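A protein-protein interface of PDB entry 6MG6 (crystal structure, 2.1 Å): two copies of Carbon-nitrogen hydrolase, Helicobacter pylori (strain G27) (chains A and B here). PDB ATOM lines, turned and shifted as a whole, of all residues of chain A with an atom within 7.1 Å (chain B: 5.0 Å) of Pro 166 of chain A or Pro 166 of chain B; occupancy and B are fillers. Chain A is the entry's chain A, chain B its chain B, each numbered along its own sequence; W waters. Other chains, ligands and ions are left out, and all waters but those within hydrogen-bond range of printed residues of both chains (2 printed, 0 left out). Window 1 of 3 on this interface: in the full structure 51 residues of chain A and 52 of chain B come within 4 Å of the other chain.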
ATOM      1  N   ASP A 162      23.805  26.068  12.812  1.00  0.00           N
ATOM      2  CA  ASP A 162      23.087  25.312  11.772  1.00  0.00           C
ATOM      3  C   ASP A 162      21.582  25.553  11.829  1.00  0.00           C
ATOM      4  O   ASP A 162      20.875  25.344  10.835  1.00  0.00           O
ATOM      5  CB  ASP A 162      23.311  23.795  11.940  1.00  0.00           C
ATOM      6  CG  ASP A 162      24.702  23.344  11.541  1.00  0.00           C
ATOM      7  OD1 ASP A 162      25.313  23.970  10.644  1.00  0.00           O
ATOM      8  OD2 ASP A 162      25.193  22.355  12.138  1.00  0.00           O
ATOM      9  N   GLN A 163      21.062  25.875  13.016  1.00  0.00           N
ATOM     10  CA  GLN A 163      19.628  25.957  13.245  1.00  0.00           C
ATOM     11  C   GLN A 163      19.004  27.183  12.597  1.00  0.00           C
ATOM     12  O   GLN A 163      17.779  27.317  12.629  1.00  0.00           O
ATOM     13  CB  GLN A 163      19.331  25.941  14.754  1.00  0.00           C
ATOM     14  CG  GLN A 163      19.625  27.251  15.459  1.00  0.00           C
ATOM     15  CD  GLN A 163      20.130  27.056  16.889  1.00  0.00           C
ATOM     16  OE1 GLN A 163      20.893  27.880  17.399  1.00  0.00           O
ATOM     17  NE2 GLN A 163      19.700  25.972  17.538  1.00  0.00           N
ATOM     18  N   TRP A 164      19.803  28.093  12.039  1.00  0.00           N
ATOM     19  CA  TRP A 164      19.232  29.238  11.328  1.00  0.00           C
ATOM     20  C   TRP A 164      19.034  28.972   9.839  1.00  0.00           C
ATOM     21  O   TRP A 164      18.554  29.869   9.113  1.00  0.00           O
ATOM     22  CB  TRP A 164      20.107  30.471  11.519  1.00  0.00           C
ATOM     23  CG  TRP A 164      20.276  30.875  12.981  1.00  0.00           C
ATOM     24  CD1 TRP A 164      21.274  30.477  13.806  1.00  0.00           C
ATOM     25  CD2 TRP A 164      19.463  31.785  13.743  1.00  0.00           C
ATOM     26  NE1 TRP A 164      21.131  31.045  15.042  1.00  0.00           N
ATOM     27  CE2 TRP A 164      20.022  31.853  15.033  1.00  0.00           C
ATOM     28  CE3 TRP A 164      18.303  32.527  13.466  1.00  0.00           C
ATOM     29  CZ2 TRP A 164      19.484  32.639  16.039  1.00  0.00           C
ATOM     30  CZ3 TRP A 164      17.775  33.316  14.464  1.00  0.00           C
ATOM     31  CH2 TRP A 164      18.362  33.367  15.745  1.00  0.00           C
ATOM     32  N   TYR A 165      19.363  27.764   9.381  1.00  0.00           N
ATOM     33  CA  TYR A 165      19.380  27.420   7.958  1.00  0.00           C
ATOM     34  C   TYR A 165      18.306  26.387   7.635  1.00  0.00           C
ATOM     35  O   TYR A 165      18.461  25.207   7.965  1.00  0.00           O
ATOM     36  CB  TYR A 165      20.766  26.903   7.564  1.00  0.00           C
ATOM     37  CG  TYR A 165      21.783  27.980   7.768  1.00  0.00           C
ATOM     38  CD1 TYR A 165      22.070  28.897   6.762  1.00  0.00           C
ATOM     39  CD2 TYR A 165      22.395  28.139   9.001  1.00  0.00           C
ATOM     40  CE1 TYR A 165      22.994  29.941   6.973  1.00  0.00           C
ATOM     41  CE2 TYR A 165      23.275  29.168   9.234  1.00  0.00           C
ATOM     42  CZ  TYR A 165      23.584  30.057   8.217  1.00  0.00           C
ATOM     43  OH  TYR A 165      24.481  31.056   8.488  1.00  0.00           O
ATOM     44  N   PRO A 166      17.200  26.786   7.013  1.00  0.00           N
ATOM     45  CA  PRO A 166      16.182  25.809   6.612  1.00  0.00           C
ATOM     46  C   PRO A 166      16.729  24.741   5.687  1.00  0.00           C
ATOM     47  O   PRO A 166      16.226  23.608   5.700  1.00  0.00           O
ATOM     48  CB  PRO A 166      15.132  26.673   5.894  1.00  0.00           C
ATOM     49  CG  PRO A 166      15.391  28.064   6.327  1.00  0.00           C
ATOM     50  CD  PRO A 166      16.857  28.156   6.615  1.00  0.00           C
ATOM     51  N   GLU A 167      17.741  25.079   4.879  1.00  0.00           N
ATOM     52  CA  GLU A 167      18.323  24.099   3.964  1.00  0.00           C
ATOM     53  C   GLU A 167      18.828  22.874   4.713  1.00  0.00           C
ATOM     54  O   GLU A 167      18.617  21.742   4.274  1.00  0.00           O
ATOM     55  CB  GLU A 167      19.479  24.724   3.165  1.00  0.00           C
ATOM     56  CG  GLU A 167      19.062  25.795   2.153  1.00  0.00           C
ATOM     57  CD  GLU A 167      19.153  27.223   2.715  1.00  0.00           C
ATOM     58  OE1 GLU A 167      18.946  27.415   3.940  1.00  0.00           O
ATOM     59  OE2 GLU A 167      19.479  28.139   1.927  1.00  0.00           O
ATOM     60  N   ALA A 168      19.505  23.077   5.840  1.00  0.00           N
ATOM     61  CA  ALA A 168      20.085  21.937   6.548  1.00  0.00           C
ATOM     62  C   ALA A 168      18.992  21.037   7.112  1.00  0.00           C
ATOM     63  O   ALA A 168      19.077  19.808   7.014  1.00  0.00           O
ATOM     64  CB  ALA A 168      21.007  22.425   7.660  1.00  0.00           C
ATOM     65  N   ALA A 169      17.984  21.632   7.750  1.00  0.00           N
ATOM     66  CA  ALA A 169      16.870  20.848   8.279  1.00  0.00           C
ATOM     67  C   ALA A 169      16.168  20.071   7.173  1.00  0.00           C
ATOM     68  O   ALA A 169      15.793  18.909   7.364  1.00  0.00           O
ATOM     69  CB  ALA A 169      15.879  21.760   8.993  1.00  0.00           C
ATOM     70  N   ARG A 170      15.980  20.701   6.012  1.00  0.00           N
ATOM     71  CA  ARG A 170      15.328  20.030   4.886  1.00  0.00           C
ATOM     72  C   ARG A 170      16.130  18.821   4.411  1.00  0.00           C
ATOM     73  O   ARG A 170      15.572  17.745   4.161  1.00  0.00           O
ATOM     74  CB  ARG A 170      15.156  21.009   3.724  1.00  0.00           C
ATOM     75  CG  ARG A 170      14.557  20.351   2.509  1.00  0.00           C
ATOM     76  CD  ARG A 170      13.094  20.111   2.766  1.00  0.00           C
ATOM     77  NE  ARG A 170      12.270  21.246   2.352  1.00  0.00           N
ATOM     78  CZ  ARG A 170      11.041  21.490   2.797  1.00  0.00           C
ATOM     79  NH1 ARG A 170      10.488  20.706   3.705  1.00  0.00           N
ATOM     80  NH2 ARG A 170      10.344  22.506   2.303  1.00  0.00           N
ATOM     81  N   ILE A 171      17.442  18.984   4.257  1.00  0.00           N
ATOM     82  CA  ILE A 171      18.269  17.880   3.775  1.00  0.00           C
ATOM     83  C   ILE A 171      18.214  16.703   4.747  1.00  0.00           C
ATOM     84  O   ILE A 171      18.094  15.546   4.327  1.00  0.00           O
ATOM     85  CB  ILE A 171      19.706  18.372   3.528  1.00  0.00           C
ATOM     86  CG1 ILE A 171      19.725  19.319   2.320  1.00  0.00           C
ATOM     87  CG2 ILE A 171      20.622  17.208   3.300  1.00  0.00           C
ATOM     88  CD1 ILE A 171      20.999  20.176   2.221  1.00  0.00           C
ATOM     89  N   MET A 172      18.272  16.977   6.059  1.00  0.00           N
ATOM     90  CA  MET A 172      18.090  15.918   7.060  1.00  0.00           C
ATOM     91  C   MET A 172      16.752  15.217   6.865  1.00  0.00           C
ATOM     92  O   MET A 172      16.673  13.980   6.853  1.00  0.00           O
ATOM     93  CB  MET A 172      18.162  16.502   8.481  1.00  0.00           C
ATOM     94  CG  MET A 172      19.557  16.964   8.891  1.00  0.00           C
ATOM     95  SD  MET A 172      20.740  15.596   8.918  1.00  0.00           S
ATOM     96  CE  MET A 172      22.145  16.412   9.708  1.00  0.00           C
ATOM     97  N   TYR A 182      19.339  20.219  18.000  1.00  0.00           N
ATOM     98  CA  TYR A 182      20.358  21.273  17.920  1.00  0.00           C
ATOM     99  C   TYR A 182      20.890  21.678  19.288  1.00  0.00           C
ATOM    100  O   TYR A 182      20.335  22.571  19.939  1.00  0.00           O
ATOM    101  CB  TYR A 182      19.819  22.527  17.241  1.00  0.00           C
ATOM    102  CG  TYR A 182      19.213  22.403  15.851  1.00  0.00           C
ATOM    103  CD1 TYR A 182      19.971  22.641  14.714  1.00  0.00           C
ATOM    104  CD2 TYR A 182      17.852  22.131  15.689  1.00  0.00           C
ATOM    105  CE1 TYR A 182      19.395  22.578  13.434  1.00  0.00           C
ATOM    106  CE2 TYR A 182      17.267  22.078  14.429  1.00  0.00           C
ATOM    107  CZ  TYR A 182      18.039  22.314  13.309  1.00  0.00           C
ATOM    108  OH  TYR A 182      17.451  22.247  12.074  1.00  0.00           O
ATOM    109  N   ILE A 207      12.460  30.397  14.211  1.00  0.00           N
ATOM    110  CA  ILE A 207      12.987  29.812  12.991  1.00  0.00           C
ATOM    111  C   ILE A 207      13.031  28.307  13.132  1.00  0.00           C
ATOM    112  O   ILE A 207      12.801  27.582  12.164  1.00  0.00           O
ATOM    113  CB  ILE A 207      14.362  30.398  12.600  1.00  0.00           C
ATOM    114  CG1 ILE A 207      14.729  29.894  11.196  1.00  0.00           C
ATOM    115  CG2 ILE A 207      15.452  30.007  13.599  1.00  0.00           C
ATOM    116  CD1 ILE A 207      15.372  30.915  10.309  1.00  0.00           C
ATOM    117  N   GLY A 210       9.818  26.641  12.532  1.00  0.00           N
ATOM    118  CA  GLY A 210       9.571  26.559  11.102  1.00  0.00           C
ATOM    119  C   GLY A 210      10.201  25.344  10.455  1.00  0.00           C
ATOM    120  O   GLY A 210       9.662  24.812   9.481  1.00  0.00           O
ATOM    121  N   HIS A 211      11.368  24.921  10.942  1.00  0.00           N
ATOM    122  CA  HIS A 211      11.965  23.682  10.449  1.00  0.00           C
ATOM    123  C   HIS A 211      11.058  22.505  10.750  1.00  0.00           C
ATOM    124  O   HIS A 211      10.875  21.618   9.908  1.00  0.00           O
ATOM    125  CB  HIS A 211      13.330  23.425  11.082  1.00  0.00           C
ATOM    126  CG  HIS A 211      14.320  24.536  10.917  1.00  0.00           C
ATOM    127  ND1 HIS A 211      14.234  25.479   9.920  1.00  0.00           N
ATOM    128  CD2 HIS A 211      15.404  24.869  11.661  1.00  0.00           C
ATOM    129  CE1 HIS A 211      15.239  26.331  10.035  1.00  0.00           C
ATOM    130  NE2 HIS A 211      15.957  25.988  11.091  1.00  0.00           N
ATOM    131  N   ALA A 214       8.003  22.794   8.407  1.00  0.00           N
ATOM    132  CA  ALA A 214       8.273  22.577   6.997  1.00  0.00           C
ATOM    133  C   ALA A 214       8.504  21.101   6.711  1.00  0.00           C
ATOM    134  O   ALA A 214       8.179  20.612   5.623  1.00  0.00           O
ATOM    135  CB  ALA A 214       9.477  23.411   6.565  1.00  0.00           C
ATOM    136  N   ASN A 215       9.036  20.370   7.684  1.00  0.00           N
ATOM    137  CA  ASN A 215       9.412  18.985   7.480  1.00  0.00           C
ATOM    138  C   ASN A 215       8.519  18.014   8.243  1.00  0.00           C
ATOM    139  O   ASN A 215       8.700  16.800   8.113  1.00  0.00           O
ATOM    140  CB  ASN A 215      10.886  18.809   7.850  1.00  0.00           C
ATOM    141  CG  ASN A 215      11.775  19.705   7.000  1.00  0.00           C
ATOM    142  OD1 ASN A 215      11.884  19.488   5.794  1.00  0.00           O
ATOM    143  ND2 ASN A 215      12.363  20.754   7.607  1.00  0.00           N
ATOM    144  N   TYR A 292      14.645  24.532  -7.893  1.00  0.00           N
ATOM    145  CA  TYR A 292      15.402  24.829  -6.679  1.00  0.00           C
ATOM    146  C   TYR A 292      16.886  25.008  -6.934  1.00  0.00           C
ATOM    147  O   TYR A 292      17.630  25.279  -5.993  1.00  0.00           O
ATOM    148  CB  TYR A 292      15.222  23.726  -5.635  1.00  0.00           C
ATOM    149  CG  TYR A 292      13.888  23.749  -4.921  1.00  0.00           C
ATOM    150  CD1 TYR A 292      12.970  24.771  -5.138  1.00  0.00           C
ATOM    151  CD2 TYR A 292      13.540  22.728  -4.043  1.00  0.00           C
ATOM    152  CE1 TYR A 292      11.711  24.776  -4.474  1.00  0.00           C
ATOM    153  CE2 TYR A 292      12.310  22.720  -3.409  1.00  0.00           C
ATOM    154  CZ  TYR A 292      11.408  23.737  -3.615  1.00  0.00           C
ATOM    155  OH  TYR A 292      10.208  23.677  -2.924  1.00  0.00           O
ATOM    156  N   LEU A 295      19.289  27.600  -5.289  1.00  0.00           N
ATOM    157  CA  LEU A 295      19.738  27.493  -3.906  1.00  0.00           C
ATOM    158  C   LEU A 295      21.226  27.212  -3.818  1.00  0.00           C
ATOM    159  O   LEU A 295      21.833  27.427  -2.758  1.00  0.00           O
ATOM    160  CB  LEU A 295      18.963  26.389  -3.190  1.00  0.00           C
ATOM    161  CG  LEU A 295      17.484  26.719  -3.019  1.00  0.00           C
ATOM    162  CD1 LEU A 295      16.694  25.459  -2.688  1.00  0.00           C
ATOM    163  CD2 LEU A 295      17.332  27.759  -1.906  1.00  0.00           C
ATOM    164  N   TRP B 164       4.734  28.043   2.471  1.00  0.00           N
ATOM    165  CA  TRP B 164       5.190  26.951   3.323  1.00  0.00           C
ATOM    166  C   TRP B 164       6.575  26.426   2.939  1.00  0.00           C
ATOM    167  O   TRP B 164       7.078  25.511   3.612  1.00  0.00           O
ATOM    168  CB  TRP B 164       4.182  25.797   3.288  1.00  0.00           C
ATOM    169  CG  TRP B 164       2.781  26.189   3.756  1.00  0.00           C
ATOM    170  CD1 TRP B 164       1.735  26.593   2.972  1.00  0.00           C
ATOM    171  CD2 TRP B 164       2.301  26.211   5.108  1.00  0.00           C
ATOM    172  NE1 TRP B 164       0.617  26.843   3.748  1.00  0.00           N
ATOM    173  CE2 TRP B 164       0.944  26.624   5.065  1.00  0.00           C
ATOM    174  CE3 TRP B 164       2.881  25.911   6.349  1.00  0.00           C
ATOM    175  CZ2 TRP B 164       0.167  26.761   6.210  1.00  0.00           C
ATOM    176  CZ3 TRP B 164       2.103  26.039   7.494  1.00  0.00           C
ATOM    177  CH2 TRP B 164       0.747  26.461   7.411  1.00  0.00           C
ATOM    178  N   TYR B 165       7.203  26.989   1.899  1.00  0.00           N
ATOM    179  CA  TYR B 165       8.453  26.476   1.342  1.00  0.00           C
ATOM    180  C   TYR B 165       9.598  27.446   1.602  1.00  0.00           C
ATOM    181  O   TYR B 165       9.705  28.477   0.927  1.00  0.00           O
ATOM    182  CB  TYR B 165       8.300  26.199  -0.167  1.00  0.00           C
ATOM    183  CG  TYR B 165       7.244  25.137  -0.365  1.00  0.00           C
ATOM    184  CD1 TYR B 165       7.593  23.790  -0.348  1.00  0.00           C
ATOM    185  CD2 TYR B 165       5.882  25.474  -0.461  1.00  0.00           C
ATOM    186  CE1 TYR B 165       6.624  22.794  -0.453  1.00  0.00           C
ATOM    187  CE2 TYR B 165       4.912  24.485  -0.543  1.00  0.00           C
ATOM    188  CZ  TYR B 165       5.302  23.142  -0.558  1.00  0.00           C
ATOM    189  OH  TYR B 165       4.375  22.121  -0.662  1.00  0.00           O
ATOM    190  N   PRO B 166      10.481  27.154   2.565  1.00  0.00           N
ATOM    191  CA  PRO B 166      11.655  28.016   2.783  1.00  0.00           C
ATOM    192  C   PRO B 166      12.497  28.199   1.533  1.00  0.00           C
ATOM    193  O   PRO B 166      13.110  29.261   1.346  1.00  0.00           O
ATOM    194  CB  PRO B 166      12.445  27.264   3.876  1.00  0.00           C
ATOM    195  CG  PRO B 166      11.456  26.376   4.526  1.00  0.00           C
ATOM    196  CD  PRO B 166      10.432  26.007   3.492  1.00  0.00           C
ATOM    197  N   GLU B 167      12.529  27.186   0.663  1.00  0.00           N
ATOM    198  CA  GLU B 167      13.324  27.277  -0.557  1.00  0.00           C
ATOM    199  C   GLU B 167      12.906  28.469  -1.410  1.00  0.00           C
ATOM    200  O   GLU B 167      13.759  29.154  -1.975  1.00  0.00           O
ATOM    201  CB  GLU B 167      13.201  25.978  -1.370  1.00  0.00           C
ATOM    202  CG  GLU B 167      13.807  24.736  -0.697  1.00  0.00           C
ATOM    203  CD  GLU B 167      12.782  23.911   0.073  1.00  0.00           C
ATOM    204  OE1 GLU B 167      11.788  24.497   0.578  1.00  0.00           O
ATOM    205  OE2 GLU B 167      12.964  22.669   0.178  1.00  0.00           O
ATOM    206  N   ALA B 168      11.591  28.705  -1.543  1.00  0.00           N
ATOM    207  CA  ALA B 168      11.089  29.773  -2.410  1.00  0.00           C
ATOM    208  C   ALA B 168      11.509  31.140  -1.903  1.00  0.00           C
ATOM    209  O   ALA B 168      12.034  31.962  -2.665  1.00  0.00           O
ATOM    210  CB  ALA B 168       9.561  29.702  -2.499  1.00  0.00           C
ATOM    211  N   ALA B 169      11.307  31.394  -0.600  1.00  0.00           N
ATOM    212  CA  ALA B 169      11.743  32.662  -0.011  1.00  0.00           C
ATOM    213  C   ALA B 169      13.248  32.866  -0.172  1.00  0.00           C
ATOM    214  O   ALA B 169      13.700  33.965  -0.482  1.00  0.00           O
ATOM    215  CB  ALA B 169      11.374  32.714   1.472  1.00  0.00           C
ATOM    216  N   ARG B 170      14.036  31.810   0.022  1.00  0.00           N
ATOM    217  CA  ARG B 170      15.480  31.951  -0.083  1.00  0.00           C
ATOM    218  C   ARG B 170      15.889  32.351  -1.493  1.00  0.00           C
ATOM    219  O   ARG B 170      16.726  33.242  -1.675  1.00  0.00           O
ATOM    220  CB  ARG B 170      16.154  30.636   0.321  1.00  0.00           C
ATOM    221  CG  ARG B 170      17.643  30.685   0.201  1.00  0.00           C
ATOM    222  CD  ARG B 170      18.253  31.472   1.327  1.00  0.00           C
ATOM    223  NE  ARG B 170      18.536  30.634   2.491  1.00  0.00           N
ATOM    224  CZ  ARG B 170      18.738  31.114   3.707  1.00  0.00           C
ATOM    225  NH1 ARG B 170      18.652  32.431   3.926  1.00  0.00           N
ATOM    226  NH2 ARG B 170      19.018  30.288   4.708  1.00  0.00           N
ATOM    227  N   ILE B 207       5.774  29.811  10.080  1.00  0.00           N
ATOM    228  CA  ILE B 207       6.647  29.421   8.977  1.00  0.00           C
ATOM    229  C   ILE B 207       7.070  30.657   8.202  1.00  0.00           C
ATOM    230  O   ILE B 207       8.213  30.764   7.737  1.00  0.00           O
ATOM    231  CB  ILE B 207       5.951  28.357   8.087  1.00  0.00           C
ATOM    232  CG1 ILE B 207       6.893  27.785   7.021  1.00  0.00           C
ATOM    233  CG2 ILE B 207       4.677  28.887   7.424  1.00  0.00           C
ATOM    234  CD1 ILE B 207       7.825  26.776   7.508  1.00  0.00           C
ATOM    235  N   HIS B 211      10.791  32.693   7.257  1.00  0.00           N
ATOM    236  CA  HIS B 211      11.313  33.210   5.994  1.00  0.00           C
ATOM    237  C   HIS B 211      11.910  34.587   6.186  1.00  0.00           C
ATOM    238  O   HIS B 211      12.985  34.888   5.657  1.00  0.00           O
ATOM    239  CB  HIS B 211      10.224  33.313   4.934  1.00  0.00           C
ATOM    240  CG  HIS B 211       9.506  32.035   4.675  1.00  0.00           C
ATOM    241  ND1 HIS B 211      10.049  30.804   4.969  1.00  0.00           N
ATOM    242  CD2 HIS B 211       8.275  31.798   4.160  1.00  0.00           C
ATOM    243  CE1 HIS B 211       9.180  29.860   4.643  1.00  0.00           C
ATOM    244  NE2 HIS B 211       8.101  30.439   4.145  1.00  0.00           N
ATOM    245  N   ALA B 214      15.220  34.122   8.240  1.00  0.00           N
ATOM    246  CA  ALA B 214      16.283  33.433   7.516  1.00  0.00           C
ATOM    247  C   ALA B 214      16.943  34.343   6.493  1.00  0.00           C
ATOM    248  O   ALA B 214      18.137  34.195   6.209  1.00  0.00           O
ATOM    249  CB  ALA B 214      15.715  32.212   6.793  1.00  0.00           C
HETATM  250  O   HOH W   1      19.199  31.519   7.172  1.00  0.00           O
HETATM  251  O   HOH W   2       7.796  22.913   3.493  1.00  0.00           O
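NE of Arg 170 of chain B lies within salt-bridge range of OE2 of Glu 167 of chain A (2.7 Å). The side-chain carboxylate (OE2) of Glu 167 of chain B lies within salt-bridge range of the guanidinium group (NE) of Arg 170 of chain A, at 2.7 Å.
The backbone carbonyl oxygen of Ile 207 of chain B lies within hydrogen-bond range of a ring nitrogen (ND1) of His 211 of chain B, 3.3 Å away. The backbone carbonyl oxygen (O) of Ala 214 of chain B sits at hydrogen-bond distance from the guanidinium group (NH1) of Arg 170 of chain B, at 2.9 Å. The backbone carbonyl oxygen (O) of Ile 207 of chain A lies within hydrogen-bond range of a ring nitrogen (ND1) of His 211 of chain A (3.4 Å). O of Ala 214 of chain A sits at hydrogen-bond distance from NH1 of Arg 170 of chain A (3.0 Å). The side-chain amide oxygen of Asn 215 of chain A is in hydrogen-bond range of the guanidinium group of Arg 170 of chain A.
Among the printed residues, pairs that only touch across the chains: Tyr 165 of chain A with Arg 170 of chain B (3.9 Å), Pro 166 of chain A with Pro 166 of chain B (3.4 Å), Pro 166 of chain A with Arg 170 of chain B (3.6 Å), Arg 170 of chain A with Pro 166 of chain B (3.7 Å), Ile 207 of chain A with Ala 214 of chain B (3.8 Å), Gly 210 of chain A with Ile 207 of chain B (3.3 Å), Ala 214 of chain A with Ile 207 of chain B (3.9 Å), Tyr 292 of chain A with Tyr 165 of chain B (3.7 Å), Tyr 292 of chain A with Glu 167 of chain B (3.6 Å), Leu 295 of chain A with Glu 167 of chain B (3.6 Å) and Leu 295 of chain A with Arg 170 of chain B (3.6 Å).
Of chain B, only Pro 166 and Arg 170 come within 4 Å of Pro 166 of chain A. Of chain A, only Pro 166 (3.4 Å) and Arg 170 (3.7 Å) come within 4 Å of Pro 166 of chain B. Printed residues of chain A within 4 Å of Tyr 165 of chain B: Tyr 292 (3.7 Å). Printed residues of chain B within 4 Å of Arg 170 of chain A: Pro 166 and Glu 167. Printed residues of chain B within 4 Å of Ala 214 of chain A: Ile 207 (3.9 Å). Printed residues of chain B within 4 Å of Leu 295 of chain A: Glu 167 (3.6 Å) and Arg 170 (3.6 Å). Printed residues of chain B within 4 Å of Tyr 165 of chain A: Arg 170. Ala 169 of chain B touches none of the printed residues of chain A. Ile 171 of chain A touches none of the printed residues of chain B.
Hydrophobic or aromatic side chains of chain A that line the printed part of chain B: Tyr 165, Pro 166, Ile 207, Ala 214, Tyr 292 and Leu 295. Along chain A the printed residues that touch a printed residue of chain B span positions 165 to 295. Among the printed residues, 13 pairs touch across the chains. Among the printed residues, Asp or Glu carboxylates within 4 Å of a Lys or Arg side-chain nitrogen of the other chain: Glu 167 of chain A with Arg 170 of chain B (2.7 Å) and Arg 170 of chain A with Glu 167 of chain B (2.7 Å).
Tyr 165 of chain A touches Arg 170 of chain B, but with the chains exchanged Arg 170 of chain A does not touch Tyr 165 of chain B (4.03 Å). Pro 166 of chain A touches Arg 170 of chain B, and with the chains exchanged Arg 170 of chain A touches Pro 166 of chain B. Glu 167 of chain A touches Arg 170 of chain B, and with the chains exchanged Arg 170 of chain A touches Glu 167 of chain B. Ile 207 of chain A touches Ala 214 of chain B, and with the chains exchanged Ala 214 of chain A touches Ile 207 of chain B. Of the 13 pairs that touch across the chains among the printed residues, 7 have their exchanged pair printed and touching as well.
Water W1 lies within hydrogen-bond range of O of Trp 164 of chain A, NH2 of Arg 170 of chain B and O of Ala 214 of chain B. Water W2 lies within hydrogen-bond range of O of Trp 164 of chain B (2.7 Å), NH2 of Arg 170 of chain A (2.8 Å) and O of Ala 214 of chain A (3.2 Å).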
